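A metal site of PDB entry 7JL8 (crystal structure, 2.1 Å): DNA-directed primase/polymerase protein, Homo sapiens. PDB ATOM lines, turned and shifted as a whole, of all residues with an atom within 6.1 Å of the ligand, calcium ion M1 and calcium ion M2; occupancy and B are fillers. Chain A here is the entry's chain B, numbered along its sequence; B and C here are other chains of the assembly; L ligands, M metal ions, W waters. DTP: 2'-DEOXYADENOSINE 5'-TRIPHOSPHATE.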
ATOM      1  N   GLU A  68     -12.088 -12.722 -11.645  1.00  0.00           N
ATOM      2  CA  GLU A  68     -11.508 -12.776 -12.985  1.00  0.00           C
ATOM      3  C   GLU A  68     -10.471 -13.894 -13.080  1.00  0.00           C
ATOM      4  O   GLU A  68      -9.549 -13.969 -12.264  1.00  0.00           O
ATOM      5  CB  GLU A  68     -10.864 -11.437 -13.349  1.00  0.00           C
ATOM      6  CG  GLU A  68     -11.789 -10.464 -14.056  1.00  0.00           C
ATOM      7  CD  GLU A  68     -11.086  -9.196 -14.509  1.00  0.00           C
ATOM      8  OE1 GLU A  68     -10.346  -8.586 -13.691  1.00  0.00           O
ATOM      9  OE2 GLU A  68     -11.274  -8.791 -15.672  1.00  0.00           O
ATOM     10  N   GLY A  74     -12.295 -10.765 -19.943  1.00  0.00           N
ATOM     11  CA  GLY A  74     -13.190 -10.414 -18.871  1.00  0.00           C
ATOM     12  C   GLY A  74     -13.947 -11.574 -18.265  1.00  0.00           C
ATOM     13  O   GLY A  74     -14.904 -11.352 -17.519  1.00  0.00           O
ATOM     14  N   ARG A  76     -15.394 -14.361 -16.003  1.00  0.00           N
ATOM     15  CA  ARG A  76     -15.482 -14.497 -14.549  1.00  0.00           C
ATOM     16  C   ARG A  76     -15.996 -15.863 -14.135  1.00  0.00           C
ATOM     17  O   ARG A  76     -16.732 -16.524 -14.876  1.00  0.00           O
ATOM     18  CB  ARG A  76     -16.433 -13.477 -13.899  1.00  0.00           C
ATOM     19  CG  ARG A  76     -15.966 -12.041 -13.742  1.00  0.00           C
ATOM     20  CD  ARG A  76     -16.478 -11.141 -14.839  1.00  0.00           C
ATOM     21  NE  ARG A  76     -16.263  -9.773 -14.377  1.00  0.00           N
ATOM     22  CZ  ARG A  76     -15.288  -8.970 -14.778  1.00  0.00           C
ATOM     23  NH1 ARG A  76     -14.408  -9.327 -15.718  1.00  0.00           N
ATOM     24  NH2 ARG A  76     -15.233  -7.756 -14.237  1.00  0.00           N
ATOM     25  N   TYR A 100     -14.600  -8.825  -7.647  1.00  0.00           N
ATOM     26  CA  TYR A 100     -15.625  -7.834  -7.912  1.00  0.00           C
ATOM     27  C   TYR A 100     -16.865  -8.187  -7.098  1.00  0.00           C
ATOM     28  O   TYR A 100     -17.169  -9.378  -6.909  1.00  0.00           O
ATOM     29  CB  TYR A 100     -15.984  -7.788  -9.391  1.00  0.00           C
ATOM     30  CG  TYR A 100     -14.780  -7.416 -10.290  1.00  0.00           C
ATOM     31  CD1 TYR A 100     -13.793  -8.338 -10.555  1.00  0.00           C
ATOM     32  CD2 TYR A 100     -14.658  -6.147 -10.833  1.00  0.00           C
ATOM     33  CE1 TYR A 100     -12.687  -8.014 -11.376  1.00  0.00           C
ATOM     34  CE2 TYR A 100     -13.568  -5.805 -11.655  1.00  0.00           C
ATOM     35  CZ  TYR A 100     -12.589  -6.744 -11.916  1.00  0.00           C
ATOM     36  OH  TYR A 100     -11.527  -6.382 -12.710  1.00  0.00           O
ATOM     37  N   ASP A 114     -18.580   5.815 -10.359  1.00  0.00           N
ATOM     38  CA  ASP A 114     -17.324   5.461 -11.029  1.00  0.00           C
ATOM     39  C   ASP A 114     -16.847   6.701 -11.797  1.00  0.00           C
ATOM     40  O   ASP A 114     -17.473   7.092 -12.789  1.00  0.00           O
ATOM     41  CB  ASP A 114     -17.507   4.268 -11.962  1.00  0.00           C
ATOM     42  CG  ASP A 114     -16.184   3.857 -12.645  1.00  0.00           C
ATOM     43  OD1 ASP A 114     -15.203   3.580 -11.944  1.00  0.00           O
ATOM     44  OD2 ASP A 114     -16.120   3.823 -13.872  1.00  0.00           O
ATOM     45  N   LEU A 115     -15.770   7.329 -11.328  1.00  0.00           N
ATOM     46  CA  LEU A 115     -15.257   8.568 -11.895  1.00  0.00           C
ATOM     47  C   LEU A 115     -13.931   8.290 -12.583  1.00  0.00           C
ATOM     48  O   LEU A 115     -13.071   7.581 -12.032  1.00  0.00           O
ATOM     49  CB  LEU A 115     -15.072   9.645 -10.827  1.00  0.00           C
ATOM     50  CG  LEU A 115     -16.251   9.822  -9.853  1.00  0.00           C
ATOM     51  CD1 LEU A 115     -15.902  10.779  -8.732  1.00  0.00           C
ATOM     52  CD2 LEU A 115     -17.502  10.330 -10.592  1.00  0.00           C
ATOM     53  N   GLU A 116     -13.754   8.866 -13.778  1.00  0.00           N
ATOM     54  CA  GLU A 116     -12.535   8.600 -14.526  1.00  0.00           C
ATOM     55  C   GLU A 116     -12.357   9.624 -15.649  1.00  0.00           C
ATOM     56  O   GLU A 116     -13.317  10.182 -16.173  1.00  0.00           O
ATOM     57  CB  GLU A 116     -12.544   7.176 -15.105  1.00  0.00           C
ATOM     58  CG  GLU A 116     -13.692   6.899 -16.033  1.00  0.00           C
ATOM     59  CD  GLU A 116     -13.900   5.418 -16.293  1.00  0.00           C
ATOM     60  OE1 GLU A 116     -13.421   4.557 -15.477  1.00  0.00           O
ATOM     61  OE2 GLU A 116     -14.551   5.090 -17.316  1.00  0.00           O
ATOM     62  N   SER A 160      -7.779   4.395  -7.658  1.00  0.00           N
ATOM     63  CA  SER A 160      -7.043   3.388  -8.436  1.00  0.00           C
ATOM     64  C   SER A 160      -6.330   4.055  -9.623  1.00  0.00           C
ATOM     65  O   SER A 160      -6.210   3.466 -10.698  1.00  0.00           O
ATOM     66  CB  SER A 160      -7.980   2.296  -8.916  1.00  0.00           C
ATOM     67  OG  SER A 160      -7.286   1.285  -9.605  1.00  0.00           O
ATOM     68  N   SER A 161      -5.844   5.272  -9.398  1.00  0.00           N
ATOM     69  CA  SER A 161      -5.248   6.093 -10.458  1.00  0.00           C
ATOM     70  C   SER A 161      -3.887   5.588 -10.892  1.00  0.00           C
ATOM     71  O   SER A 161      -3.167   4.925 -10.145  1.00  0.00           O
ATOM     72  CB  SER A 161      -5.095   7.539  -9.978  1.00  0.00           C
ATOM     73  OG  SER A 161      -6.360   8.190  -9.873  1.00  0.00           O
ATOM     74  N   LYS A 165      -4.413   7.504 -16.114  1.00  0.00           N
ATOM     75  CA  LYS A 165      -5.839   7.524 -15.848  1.00  0.00           C
ATOM     76  C   LYS A 165      -6.104   8.016 -14.424  1.00  0.00           C
ATOM     77  O   LYS A 165      -5.518   7.513 -13.457  1.00  0.00           O
ATOM     78  CB  LYS A 165      -6.428   6.110 -16.051  1.00  0.00           C
ATOM     79  CG  LYS A 165      -7.940   6.053 -15.938  1.00  0.00           C
ATOM     80  CD  LYS A 165      -8.478   4.686 -16.322  1.00  0.00           C
ATOM     81  CE  LYS A 165     -10.000   4.601 -16.157  1.00  0.00           C
ATOM     82  NZ  LYS A 165     -10.534   3.263 -16.551  1.00  0.00           N
ATOM     83  N   PHE A 166      -6.947   9.026 -14.306  1.00  0.00           N
ATOM     84  CA  PHE A 166      -7.542   9.377 -13.029  1.00  0.00           C
ATOM     85  C   PHE A 166      -8.721   8.442 -12.819  1.00  0.00           C
ATOM     86  O   PHE A 166      -9.557   8.263 -13.722  1.00  0.00           O
ATOM     87  CB  PHE A 166      -7.972  10.837 -13.013  1.00  0.00           C
ATOM     88  CG  PHE A 166      -8.552  11.295 -11.684  1.00  0.00           C
ATOM     89  CD1 PHE A 166      -7.732  11.756 -10.673  1.00  0.00           C
ATOM     90  CD2 PHE A 166      -9.912  11.250 -11.462  1.00  0.00           C
ATOM     91  CE1 PHE A 166      -8.264  12.175  -9.459  1.00  0.00           C
ATOM     92  CE2 PHE A 166     -10.458  11.672 -10.265  1.00  0.00           C
ATOM     93  CZ  PHE A 166      -9.630  12.130  -9.250  1.00  0.00           C
ATOM     94  N   SER A 167      -8.752   7.763 -11.673  1.00  0.00           N
ATOM     95  CA  SER A 167      -9.771   6.740 -11.424  1.00  0.00           C
ATOM     96  C   SER A 167     -10.154   6.767  -9.957  1.00  0.00           C
ATOM     97  O   SER A 167      -9.313   6.527  -9.091  1.00  0.00           O
ATOM     98  CB  SER A 167      -9.256   5.362 -11.825  1.00  0.00           C
ATOM     99  OG  SER A 167     -10.106   4.318 -11.382  1.00  0.00           O
ATOM    100  N   ARG A 168     -11.429   7.057  -9.682  1.00  0.00           N
ATOM    101  CA  ARG A 168     -11.970   7.037  -8.335  1.00  0.00           C
ATOM    102  C   ARG A 168     -13.268   6.249  -8.307  1.00  0.00           C
ATOM    103  O   ARG A 168     -14.044   6.253  -9.274  1.00  0.00           O
ATOM    104  CB  ARG A 168     -12.256   8.441  -7.806  1.00  0.00           C
ATOM    105  CG  ARG A 168     -11.054   9.350  -7.754  1.00  0.00           C
ATOM    106  CD  ARG A 168     -10.286   9.195  -6.452  1.00  0.00           C
ATOM    107  NE  ARG A 168      -9.067  10.013  -6.460  1.00  0.00           N
ATOM    108  CZ  ARG A 168      -8.938  11.197  -5.851  1.00  0.00           C
ATOM    109  NH1 ARG A 168      -9.955  11.754  -5.142  1.00  0.00           N
ATOM    110  NH2 ARG A 168      -7.777  11.821  -5.936  1.00  0.00           N
ATOM    111  N   HIS A 169     -13.517   5.591  -7.170  1.00  0.00           N
ATOM    112  CA  HIS A 169     -14.822   5.067  -6.812  1.00  0.00           C
ATOM    113  C   HIS A 169     -15.318   5.782  -5.568  1.00  0.00           C
ATOM    114  O   HIS A 169     -14.582   5.875  -4.562  1.00  0.00           O
ATOM    115  CB  HIS A 169     -14.769   3.581  -6.499  1.00  0.00           C
ATOM    116  CG  HIS A 169     -14.631   2.715  -7.706  1.00  0.00           C
ATOM    117  ND1 HIS A 169     -14.710   1.335  -7.631  1.00  0.00           N
ATOM    118  CD2 HIS A 169     -14.421   3.023  -9.010  1.00  0.00           C
ATOM    119  CE1 HIS A 169     -14.556   0.834  -8.840  1.00  0.00           C
ATOM    120  NE2 HIS A 169     -14.397   1.838  -9.704  1.00  0.00           N
ATOM    121  N   ASP A 280     -19.013   8.134 -14.951  1.00  0.00           N
ATOM    122  CA  ASP A 280     -19.234   7.028 -15.885  1.00  0.00           C
ATOM    123  C   ASP A 280     -20.641   6.495 -15.667  1.00  0.00           C
ATOM    124  O   ASP A 280     -20.917   5.801 -14.680  1.00  0.00           O
ATOM    125  CB  ASP A 280     -18.186   5.946 -15.667  1.00  0.00           C
ATOM    126  CG  ASP A 280     -18.418   4.737 -16.531  1.00  0.00           C
ATOM    127  OD1 ASP A 280     -19.274   4.794 -17.432  1.00  0.00           O
ATOM    128  OD2 ASP A 280     -17.727   3.720 -16.315  1.00  0.00           O
ATOM    129  N   VAL A 283     -22.167   2.198 -15.445  1.00  0.00           N
ATOM    130  CA  VAL A 283     -22.098   1.189 -14.397  1.00  0.00           C
ATOM    131  C   VAL A 283     -23.428   1.013 -13.679  1.00  0.00           C
ATOM    132  O   VAL A 283     -23.489   0.373 -12.613  1.00  0.00           O
ATOM    133  CB  VAL A 283     -20.991   1.515 -13.389  1.00  0.00           C
ATOM    134  CG1 VAL A 283     -19.652   1.544 -14.091  1.00  0.00           C
ATOM    135  CG2 VAL A 283     -21.265   2.841 -12.693  1.00  0.00           C
ATOM    136  N   ARG A 288     -24.340  -5.383 -12.310  1.00  0.00           N
ATOM    137  CA  ARG A 288     -23.058  -4.754 -12.559  1.00  0.00           C
ATOM    138  C   ARG A 288     -22.024  -5.241 -11.549  1.00  0.00           C
ATOM    139  O   ARG A 288     -22.273  -5.246 -10.329  1.00  0.00           O
ATOM    140  CB  ARG A 288     -23.203  -3.226 -12.504  1.00  0.00           C
ATOM    141  CG  ARG A 288     -21.920  -2.388 -12.354  1.00  0.00           C
ATOM    142  CD  ARG A 288     -20.980  -2.439 -13.595  1.00  0.00           C
ATOM    143  NE  ARG A 288     -21.744  -2.396 -14.841  1.00  0.00           N
ATOM    144  CZ  ARG A 288     -21.209  -2.456 -16.059  1.00  0.00           C
ATOM    145  NH1 ARG A 288     -19.886  -2.537 -16.221  1.00  0.00           N
ATOM    146  NH2 ARG A 288     -22.021  -2.454 -17.102  1.00  0.00           N
ATOM    147  N   ASN A 289     -20.869  -5.632 -12.101  1.00  0.00           N
ATOM    148  CA  ASN A 289     -19.745  -5.879 -11.280  1.00  0.00           C
ATOM    149  C   ASN A 289     -19.072  -4.585 -10.847  1.00  0.00           C
ATOM    150  O   ASN A 289     -19.021  -3.610 -11.622  1.00  0.00           O
ATOM    151  CB  ASN A 289     -18.627  -6.829 -11.783  1.00  0.00           C
ATOM    152  CG  ASN A 289     -19.096  -8.268 -12.096  1.00  0.00           C
ATOM    153  OD1 ASN A 289     -18.429  -8.893 -12.875  1.00  0.00           O
ATOM    154  ND2 ASN A 289     -20.444  -8.444 -12.109  1.00  0.00           N
ATOM    155  N   PHE A 290     -18.479  -4.567  -9.633  1.00  0.00           N
ATOM    156  CA  PHE A 290     -17.851  -3.322  -9.163  1.00  0.00           C
ATOM    157  C   PHE A 290     -16.649  -3.720  -8.303  1.00  0.00           C
ATOM    158  O   PHE A 290     -16.809  -4.299  -7.224  1.00  0.00           O
ATOM    159  CB  PHE A 290     -18.842  -2.464  -8.373  1.00  0.00           C
ATOM    160  CG  PHE A 290     -18.511  -0.975  -8.356  1.00  0.00           C
ATOM    161  CD1 PHE A 290     -18.424  -0.254  -9.546  1.00  0.00           C
ATOM    162  CD2 PHE A 290     -18.325  -0.301  -7.176  1.00  0.00           C
ATOM    163  CE1 PHE A 290     -18.137   1.093  -9.544  1.00  0.00           C
ATOM    164  CE2 PHE A 290     -18.018   1.070  -7.177  1.00  0.00           C
ATOM    165  CZ  PHE A 290     -17.925   1.758  -8.352  1.00  0.00           C
ATOM    166  N   ARG A 291     -15.460  -3.396  -8.820  1.00  0.00           N
ATOM    167  CA  ARG A 291     -14.220  -3.958  -8.331  1.00  0.00           C
ATOM    168  C   ARG A 291     -14.055  -3.696  -6.842  1.00  0.00           C
ATOM    169  O   ARG A 291     -14.352  -2.610  -6.339  1.00  0.00           O
ATOM    170  CB  ARG A 291     -13.043  -3.367  -9.123  1.00  0.00           C
ATOM    171  CG  ARG A 291     -11.719  -3.885  -8.659  1.00  0.00           C
ATOM    172  CD  ARG A 291     -10.582  -3.607  -9.610  1.00  0.00           C
ATOM    173  NE  ARG A 291     -10.556  -2.247 -10.151  1.00  0.00           N
ATOM    174  CZ  ARG A 291      -9.574  -1.380  -9.949  1.00  0.00           C
ATOM    175  NH1 ARG A 291      -8.558  -1.709  -9.162  1.00  0.00           N
ATOM    176  NH2 ARG A 291      -9.619  -0.185 -10.515  1.00  0.00           N
ATOM    177  N   LYS A 297      -7.516  -5.010 -11.300  1.00  0.00           N
ATOM    178  CA  LYS A 297      -7.888  -5.737 -12.495  1.00  0.00           C
ATOM    179  C   LYS A 297      -6.816  -6.772 -12.835  1.00  0.00           C
ATOM    180  O   LYS A 297      -5.629  -6.586 -12.529  1.00  0.00           O
ATOM    181  CB  LYS A 297      -8.076  -4.784 -13.681  1.00  0.00           C
ATOM    182  CG  LYS A 297      -9.335  -3.948 -13.545  1.00  0.00           C
ATOM    183  CD  LYS A 297      -9.356  -2.786 -14.526  1.00  0.00           C
ATOM    184  CE  LYS A 297     -10.784  -2.525 -14.990  1.00  0.00           C
ATOM    185  NZ  LYS A 297     -10.873  -1.429 -15.999  1.00  0.00           N
ATOM    186  N   VAL A 302      -2.635  -2.044  -9.938  1.00  0.00           N
ATOM    187  CA  VAL A 302      -3.147  -0.959  -9.110  1.00  0.00           C
ATOM    188  C   VAL A 302      -4.462  -1.374  -8.463  1.00  0.00           C
ATOM    189  O   VAL A 302      -5.463  -1.635  -9.139  1.00  0.00           O
ATOM    190  CB  VAL A 302      -3.314   0.351  -9.903  1.00  0.00           C
ATOM    191  CG1 VAL A 302      -4.314   0.191 -11.042  1.00  0.00           C
ATOM    192  CG2 VAL A 302      -3.773   1.459  -8.968  1.00  0.00           C
ATOM    193  N   LEU A 304      -7.655  -0.731  -5.680  1.00  0.00           N
ATOM    194  CA  LEU A 304      -8.460   0.318  -5.051  1.00  0.00           C
ATOM    195  C   LEU A 304      -8.055   0.451  -3.583  1.00  0.00           C
ATOM    196  O   LEU A 304      -8.144  -0.520  -2.822  1.00  0.00           O
ATOM    197  CB  LEU A 304      -9.952  -0.009  -5.173  1.00  0.00           C
ATOM    198  CG  LEU A 304     -10.573   0.296  -6.554  1.00  0.00           C
ATOM    199  CD1 LEU A 304     -11.803  -0.566  -6.790  1.00  0.00           C
ATOM    200  CD2 LEU A 304     -10.950   1.785  -6.734  1.00  0.00           C
ATOM    201  P    DT B   3     -17.495 -17.237 -20.671  1.00  0.00           P
ATOM    202  OP1  DT B   3     -17.331 -18.605 -20.125  1.00  0.00           O
ATOM    203  OP2  DT B   3     -18.681 -16.834 -21.484  1.00  0.00           O
ATOM    204  O5'  DT B   3     -17.475 -16.249 -19.407  1.00  0.00           O
ATOM    205  C5'  DT B   3     -17.685 -16.751 -18.106  1.00  0.00           C
ATOM    206  C4'  DT B   3     -18.646 -15.851 -17.323  1.00  0.00           C
ATOM    207  O4'  DT B   3     -18.110 -14.511 -17.241  1.00  0.00           O
ATOM    208  C3'  DT B   3     -20.025 -15.707 -17.938  1.00  0.00           C
ATOM    209  O3'  DT B   3     -21.037 -15.777 -16.918  1.00  0.00           O
ATOM    210  C2'  DT B   3     -20.001 -14.342 -18.649  1.00  0.00           C
ATOM    211  C1'  DT B   3     -19.037 -13.552 -17.776  1.00  0.00           C
ATOM    212  N1   DT B   3     -18.247 -12.487 -18.480  1.00  0.00           N
ATOM    213  C2   DT B   3     -18.267 -11.195 -17.993  1.00  0.00           C
ATOM    214  O2   DT B   3     -18.894 -10.844 -17.006  1.00  0.00           O
ATOM    215  N3   DT B   3     -17.514 -10.308 -18.707  1.00  0.00           N
ATOM    216  C4   DT B   3     -16.762 -10.569 -19.824  1.00  0.00           C
ATOM    217  O4   DT B   3     -16.129  -9.702 -20.389  1.00  0.00           O
ATOM    218  C5   DT B   3     -16.774 -11.940 -20.279  1.00  0.00           C
ATOM    219  C7   DT B   3     -15.998 -12.327 -21.497  1.00  0.00           C
ATOM    220  C6   DT B   3     -17.507 -12.824 -19.605  1.00  0.00           C
ATOM    221  P   8OG B   4     -22.571 -15.886 -17.338  1.00  0.00           P
ATOM    222  OP1 8OG B   4     -23.329 -16.536 -16.216  1.00  0.00           O
ATOM    223  OP2 8OG B   4     -22.622 -16.712 -18.607  1.00  0.00           O
ATOM    224  O5' 8OG B   4     -23.062 -14.361 -17.544  1.00  0.00           O
ATOM    225  C5' 8OG B   4     -23.149 -13.569 -16.405  1.00  0.00           C
ATOM    226  C4' 8OG B   4     -23.529 -12.157 -16.768  1.00  0.00           C
ATOM    227  O4' 8OG B   4     -22.312 -11.510 -17.580  1.00  0.00           O
ATOM    228  C3' 8OG B   4     -24.608 -12.009 -17.537  1.00  0.00           C
ATOM    229  O3' 8OG B   4     -25.482 -11.066 -16.733  1.00  0.00           O
ATOM    230  C2' 8OG B   4     -24.123 -11.410 -18.836  1.00  0.00           C
ATOM    231  C1' 8OG B   4     -22.884 -10.649 -18.391  1.00  0.00           C
ATOM    232  N9  8OG B   4     -21.869 -10.369 -19.380  1.00  0.00           N
ATOM    233  C8  8OG B   4     -21.354 -11.285 -20.440  1.00  0.00           C
ATOM    234  N7  8OG B   4     -20.268 -10.510 -21.164  1.00  0.00           N
ATOM    235  C5  8OG B   4     -20.180  -9.210 -20.524  1.00  0.00           C
ATOM    236  C6  8OG B   4     -19.286  -8.029 -20.828  1.00  0.00           C
ATOM    237  O6  8OG B   4     -18.502  -8.067 -21.710  1.00  0.00           O
ATOM    238  N1  8OG B   4     -19.410  -6.847 -20.018  1.00  0.00           N
ATOM    239  C2  8OG B   4     -20.408  -6.815 -18.922  1.00  0.00           C
ATOM    240  N2  8OG B   4     -20.529  -5.642 -18.096  1.00  0.00           N
ATOM    241  N3  8OG B   4     -21.244  -7.926 -18.638  1.00  0.00           N
ATOM    242  C4  8OG B   4     -21.112  -9.139 -19.467  1.00  0.00           C
ATOM    243  O8  8OG B   4     -21.747 -12.412 -20.672  1.00  0.00           O
ATOM    244  P    DC C  13     -15.000   2.524 -21.717  1.00  0.00           P
ATOM    245  OP1  DC C  13     -15.189   3.982 -21.569  1.00  0.00           O
ATOM    246  OP2  DC C  13     -13.648   1.938 -21.809  1.00  0.00           O
ATOM    247  O5'  DC C  13     -15.749   1.741 -20.518  1.00  0.00           O
ATOM    248  C5'  DC C  13     -17.062   2.134 -20.127  1.00  0.00           C
ATOM    249  C4'  DC C  13     -17.710   1.081 -19.238  1.00  0.00           C
ATOM    250  O4'  DC C  13     -17.858  -0.120 -20.001  1.00  0.00           O
ATOM    251  C3'  DC C  13     -16.928   0.687 -18.007  1.00  0.00           C
ATOM    252  O3'  DC C  13     -17.522   1.260 -16.839  1.00  0.00           O
ATOM    253  C2'  DC C  13     -16.977  -0.858 -17.949  1.00  0.00           C
ATOM    254  C1'  DC C  13     -17.919  -1.195 -19.102  1.00  0.00           C
ATOM    255  N1   DC C  13     -17.537  -2.387 -19.828  1.00  0.00           N
ATOM    256  C2   DC C  13     -18.248  -3.570 -19.601  1.00  0.00           C
ATOM    257  O2   DC C  13     -19.180  -3.561 -18.798  1.00  0.00           O
ATOM    258  N3   DC C  13     -17.883  -4.692 -20.259  1.00  0.00           N
ATOM    259  C4   DC C  13     -16.863  -4.654 -21.119  1.00  0.00           C
ATOM    260  N4   DC C  13     -16.557  -5.789 -21.757  1.00  0.00           N
ATOM    261  C5   DC C  13     -16.125  -3.454 -21.367  1.00  0.00           C
ATOM    262  C6   DC C  13     -16.490  -2.354 -20.701  1.00  0.00           C
HETATM  263  PG  DTP L   1     -10.369   1.636 -13.717  1.00  0.00           P
HETATM  264  O1G DTP L   1      -9.720   0.985 -14.916  1.00  0.00           O
HETATM  265  O2G DTP L   1     -11.456   2.587 -14.130  1.00  0.00           O
HETATM  266  O3G DTP L   1      -9.461   2.210 -12.632  1.00  0.00           O
HETATM  267  PB  DTP L   1     -12.649   0.111 -12.703  1.00  0.00           P
HETATM  268  O1B DTP L   1     -13.456   1.412 -12.485  1.00  0.00           O
HETATM  269  O2B DTP L   1     -12.830  -1.071 -11.777  1.00  0.00           O
HETATM  270  O3B DTP L   1     -11.059   0.350 -12.896  1.00  0.00           O
HETATM  271  PA  DTP L   1     -14.031   0.052 -15.327  1.00  0.00           P
HETATM  272  O1A DTP L   1     -13.456  -0.536 -16.596  1.00  0.00           O
HETATM  273  O2A DTP L   1     -14.370   1.510 -15.282  1.00  0.00           O
HETATM  274  O3A DTP L   1     -13.045  -0.478 -14.170  1.00  0.00           O
HETATM  275  O5' DTP L   1     -15.436  -0.708 -15.065  1.00  0.00           O
HETATM  276  C5' DTP L   1     -16.309  -0.296 -14.021  1.00  0.00           C
HETATM  277  C4' DTP L   1     -16.763  -1.587 -13.371  1.00  0.00           C
HETATM  278  O4' DTP L   1     -17.479  -2.320 -14.368  1.00  0.00           O
HETATM  279  C3' DTP L   1     -15.618  -2.486 -12.915  1.00  0.00           C
HETATM  280  O3' DTP L   1     -15.160  -2.287 -11.590  1.00  0.00           O
HETATM  281  C2' DTP L   1     -16.140  -3.888 -13.180  1.00  0.00           C
HETATM  282  C1' DTP L   1     -17.215  -3.706 -14.264  1.00  0.00           C
HETATM  283  N9  DTP L   1     -16.673  -4.262 -15.510  1.00  0.00           N
HETATM  284  C8  DTP L   1     -15.705  -3.687 -16.260  1.00  0.00           C
HETATM  285  N7  DTP L   1     -15.383  -4.468 -17.320  1.00  0.00           N
HETATM  286  C5  DTP L   1     -16.133  -5.569 -17.248  1.00  0.00           C
HETATM  287  C6  DTP L   1     -16.302  -6.802 -18.039  1.00  0.00           C
HETATM  288  N6  DTP L   1     -15.565  -6.983 -19.136  1.00  0.00           N
HETATM  289  N1  DTP L   1     -17.198  -7.731 -17.632  1.00  0.00           N
HETATM  290  C2  DTP L   1     -17.942  -7.534 -16.532  1.00  0.00           C
HETATM  291  N3  DTP L   1     -17.838  -6.433 -15.754  1.00  0.00           N
HETATM  292  C4  DTP L   1     -16.978  -5.438 -16.053  1.00  0.00           C
HETATM  293 CA    CA M   1     -15.421   3.191 -15.967  1.00  0.00          CA
HETATM  294 CA    CA M   2     -13.726   3.184 -13.757  1.00  0.00          CA
HETATM  295  O   HOH W   1     -12.761   4.321 -12.247  1.00  0.00           O
HETATM  296  O   HOH W   2     -13.896   2.834 -18.037  1.00  0.00           O
HETATM  297  O   HOH W   3      -7.093   3.127 -13.606  1.00  0.00           O
HETATM  298  O   HOH W   4     -20.523  -5.755 -14.826  1.00  0.00           O
HETATM  299  O   HOH W   5      -7.201   0.421 -13.139  1.00  0.00           O
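Water W1 bridges the side-chain hydroxyl of Ser 167 and the backbone carbonyl oxygen of Leu 115.
Water W3 bridges an oxygen (O3G) of the ligand (2.7 Å) and the backbone carbonyl oxygen (O) of Ser 160 (3.1 Å).
Water W4 lies within hydrogen-bond range of N of Asn 289 (2.7 Å), N3 of the ligand (2.9 Å) and N2 of 8OG 4 of chain B (3.3 Å).
NZ of Lys 165 is in salt-bridge range of O1G of the ligand, at 2.9 Å.
A nitrogen (N3) of the ligand lies within hydrogen-bond range of the guanidinium group (NH2) of Arg 76, 3.3 Å away.
N6 of the ligand is in hydrogen-bond range of O4 of DT 3 of chain B, at 3.0 Å.
The backbone NH (N) of Arg 291 sits at hydrogen-bond distance from an oxygen (O3') of the ligand (3.0 Å).
NZ of Lys 297 lies within salt-bridge range of O1A of the ligand (2.8 Å).
A ring nitrogen (NE2) of His 169 lies close to an oxygen (O1B) of the ligand, 3.0 Å away.
N4 of DC 13 of chain C lies within hydrogen-bond range of a nitrogen (N6) of the ligand (3.0 Å).
O4' of the ligand lies within hydrogen-bond range of NH1 of Arg 288, at 3.0 Å.
An oxygen (O2B) of the ligand lies within salt-bridge range of the guanidinium group of Arg 291 (3.0 Å).
OG of Ser 167 lies within hydrogen-bond range of O3G of the ligand, 2.5 Å away.
Calcium ion M2 is bound by water W1 (2.1 Å), an oxygen (O1B) of the ligand (2.2 Å), the side-chain carboxylate (OE1) of Glu 116 (2.2 Å), an oxygen (O2A) of the ligand (2.4 Å), the side-chain carboxylate (OD1) of Asp 114 (2.4 Å), an oxygen (O2G) of the ligand (2.4 Å) and the side-chain carboxylate (OD2) of Asp 114 (2.5 Å).
Calcium ion M2 has seven donor atoms within binding distance.
Of the 26 residues printed, 4 come within 4 Å of calcium ion M1.
Along chain A the residues within 4 Å of calcium ion M1 span positions 114 to 280.
The nearest printed residue that does not touch calcium ion M1 is Val 283 (4.9 Å).
Two residues have an atom within 4 Å of calcium ion M2: Asp 114 and Glu 116.
The nearest printed residue that does not touch calcium ion M2 is Lys 165 (4.2 Å).
A ring nitrogen (NE2) of His 169 lies close to the side-chain carboxylate (OD1) of Asp 114, at 2.9 Å.
The side-chain carboxylate (OE1) of Glu 68 sits at hydrogen-bond distance from the side-chain hydroxyl (OH) of Tyr 100 (2.7 Å).
O4' of DT 3 of chain B is in hydrogen-bond range of the backbone NH (N) of Arg 76 (3.0 Å).
O2 of DC 13 of chain C lies close to N2 of 8OG 4 of chain B, at 2.6 Å.
The side-chain amide oxygen of Asn 289 is in hydrogen-bond range of the guanidinium group of Arg 76.
The backbone carbonyl oxygen of Val 302 lies within hydrogen-bond range of the guanidinium group of Arg 291 (3.1 Å).
O2 of DC 13 of chain C sits at hydrogen-bond distance from NH1 of Arg 288.
The side-chain carboxylate (OE2) of Glu 68 is in salt-bridge range of the guanidinium group (NH1) of Arg 76 (3.2 Å).
The backbone carbonyl oxygen (O) of Asn 289 sits close to an oxygen (O4') of the ligand, at 3.4 Å.
N1 of 8OG 4 of chain B sits close to a nitrogen (N1) of the ligand, 3.4 Å away.
Merely in contact with the ligand: Tyr 100 (3.6 Å), Ser 160 (3.8 Å), Val 283 (3.8 Å) and Phe 290 (3.8 Å).
Within 4 Å of the ligand: Arg 76, Tyr 100, Asp 114, Glu 116, Ser 160, Lys 165, Ser 167, His 169, Val 283, Arg 288, Asn 289, Phe 290, Arg 291, Lys 297, DT 3 of chain B, 8OG 4 of chain B and DC 13 of chain C.
An oxygen (O2A) of the ligand binds calcium ion M1.
OD2 of Asp 114 is bound to calcium ion M1 (2.3 Å).
OD2 of Asp 280 is bound to calcium ion M1, at 2.4 Å.
OE1 of Glu 116 is bound to calcium ion M1 (2.5 Å).
OE2 of Glu 116 binds calcium ion M1, 2.5 Å away.
Water W2 is bound to calcium ion M1 (2.6 Å).
Calcium ion M1 has six donor atoms within binding distance.
Slightly farther from calcium ion M1 lies O3' of DC 13 of chain C (3.0 Å).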
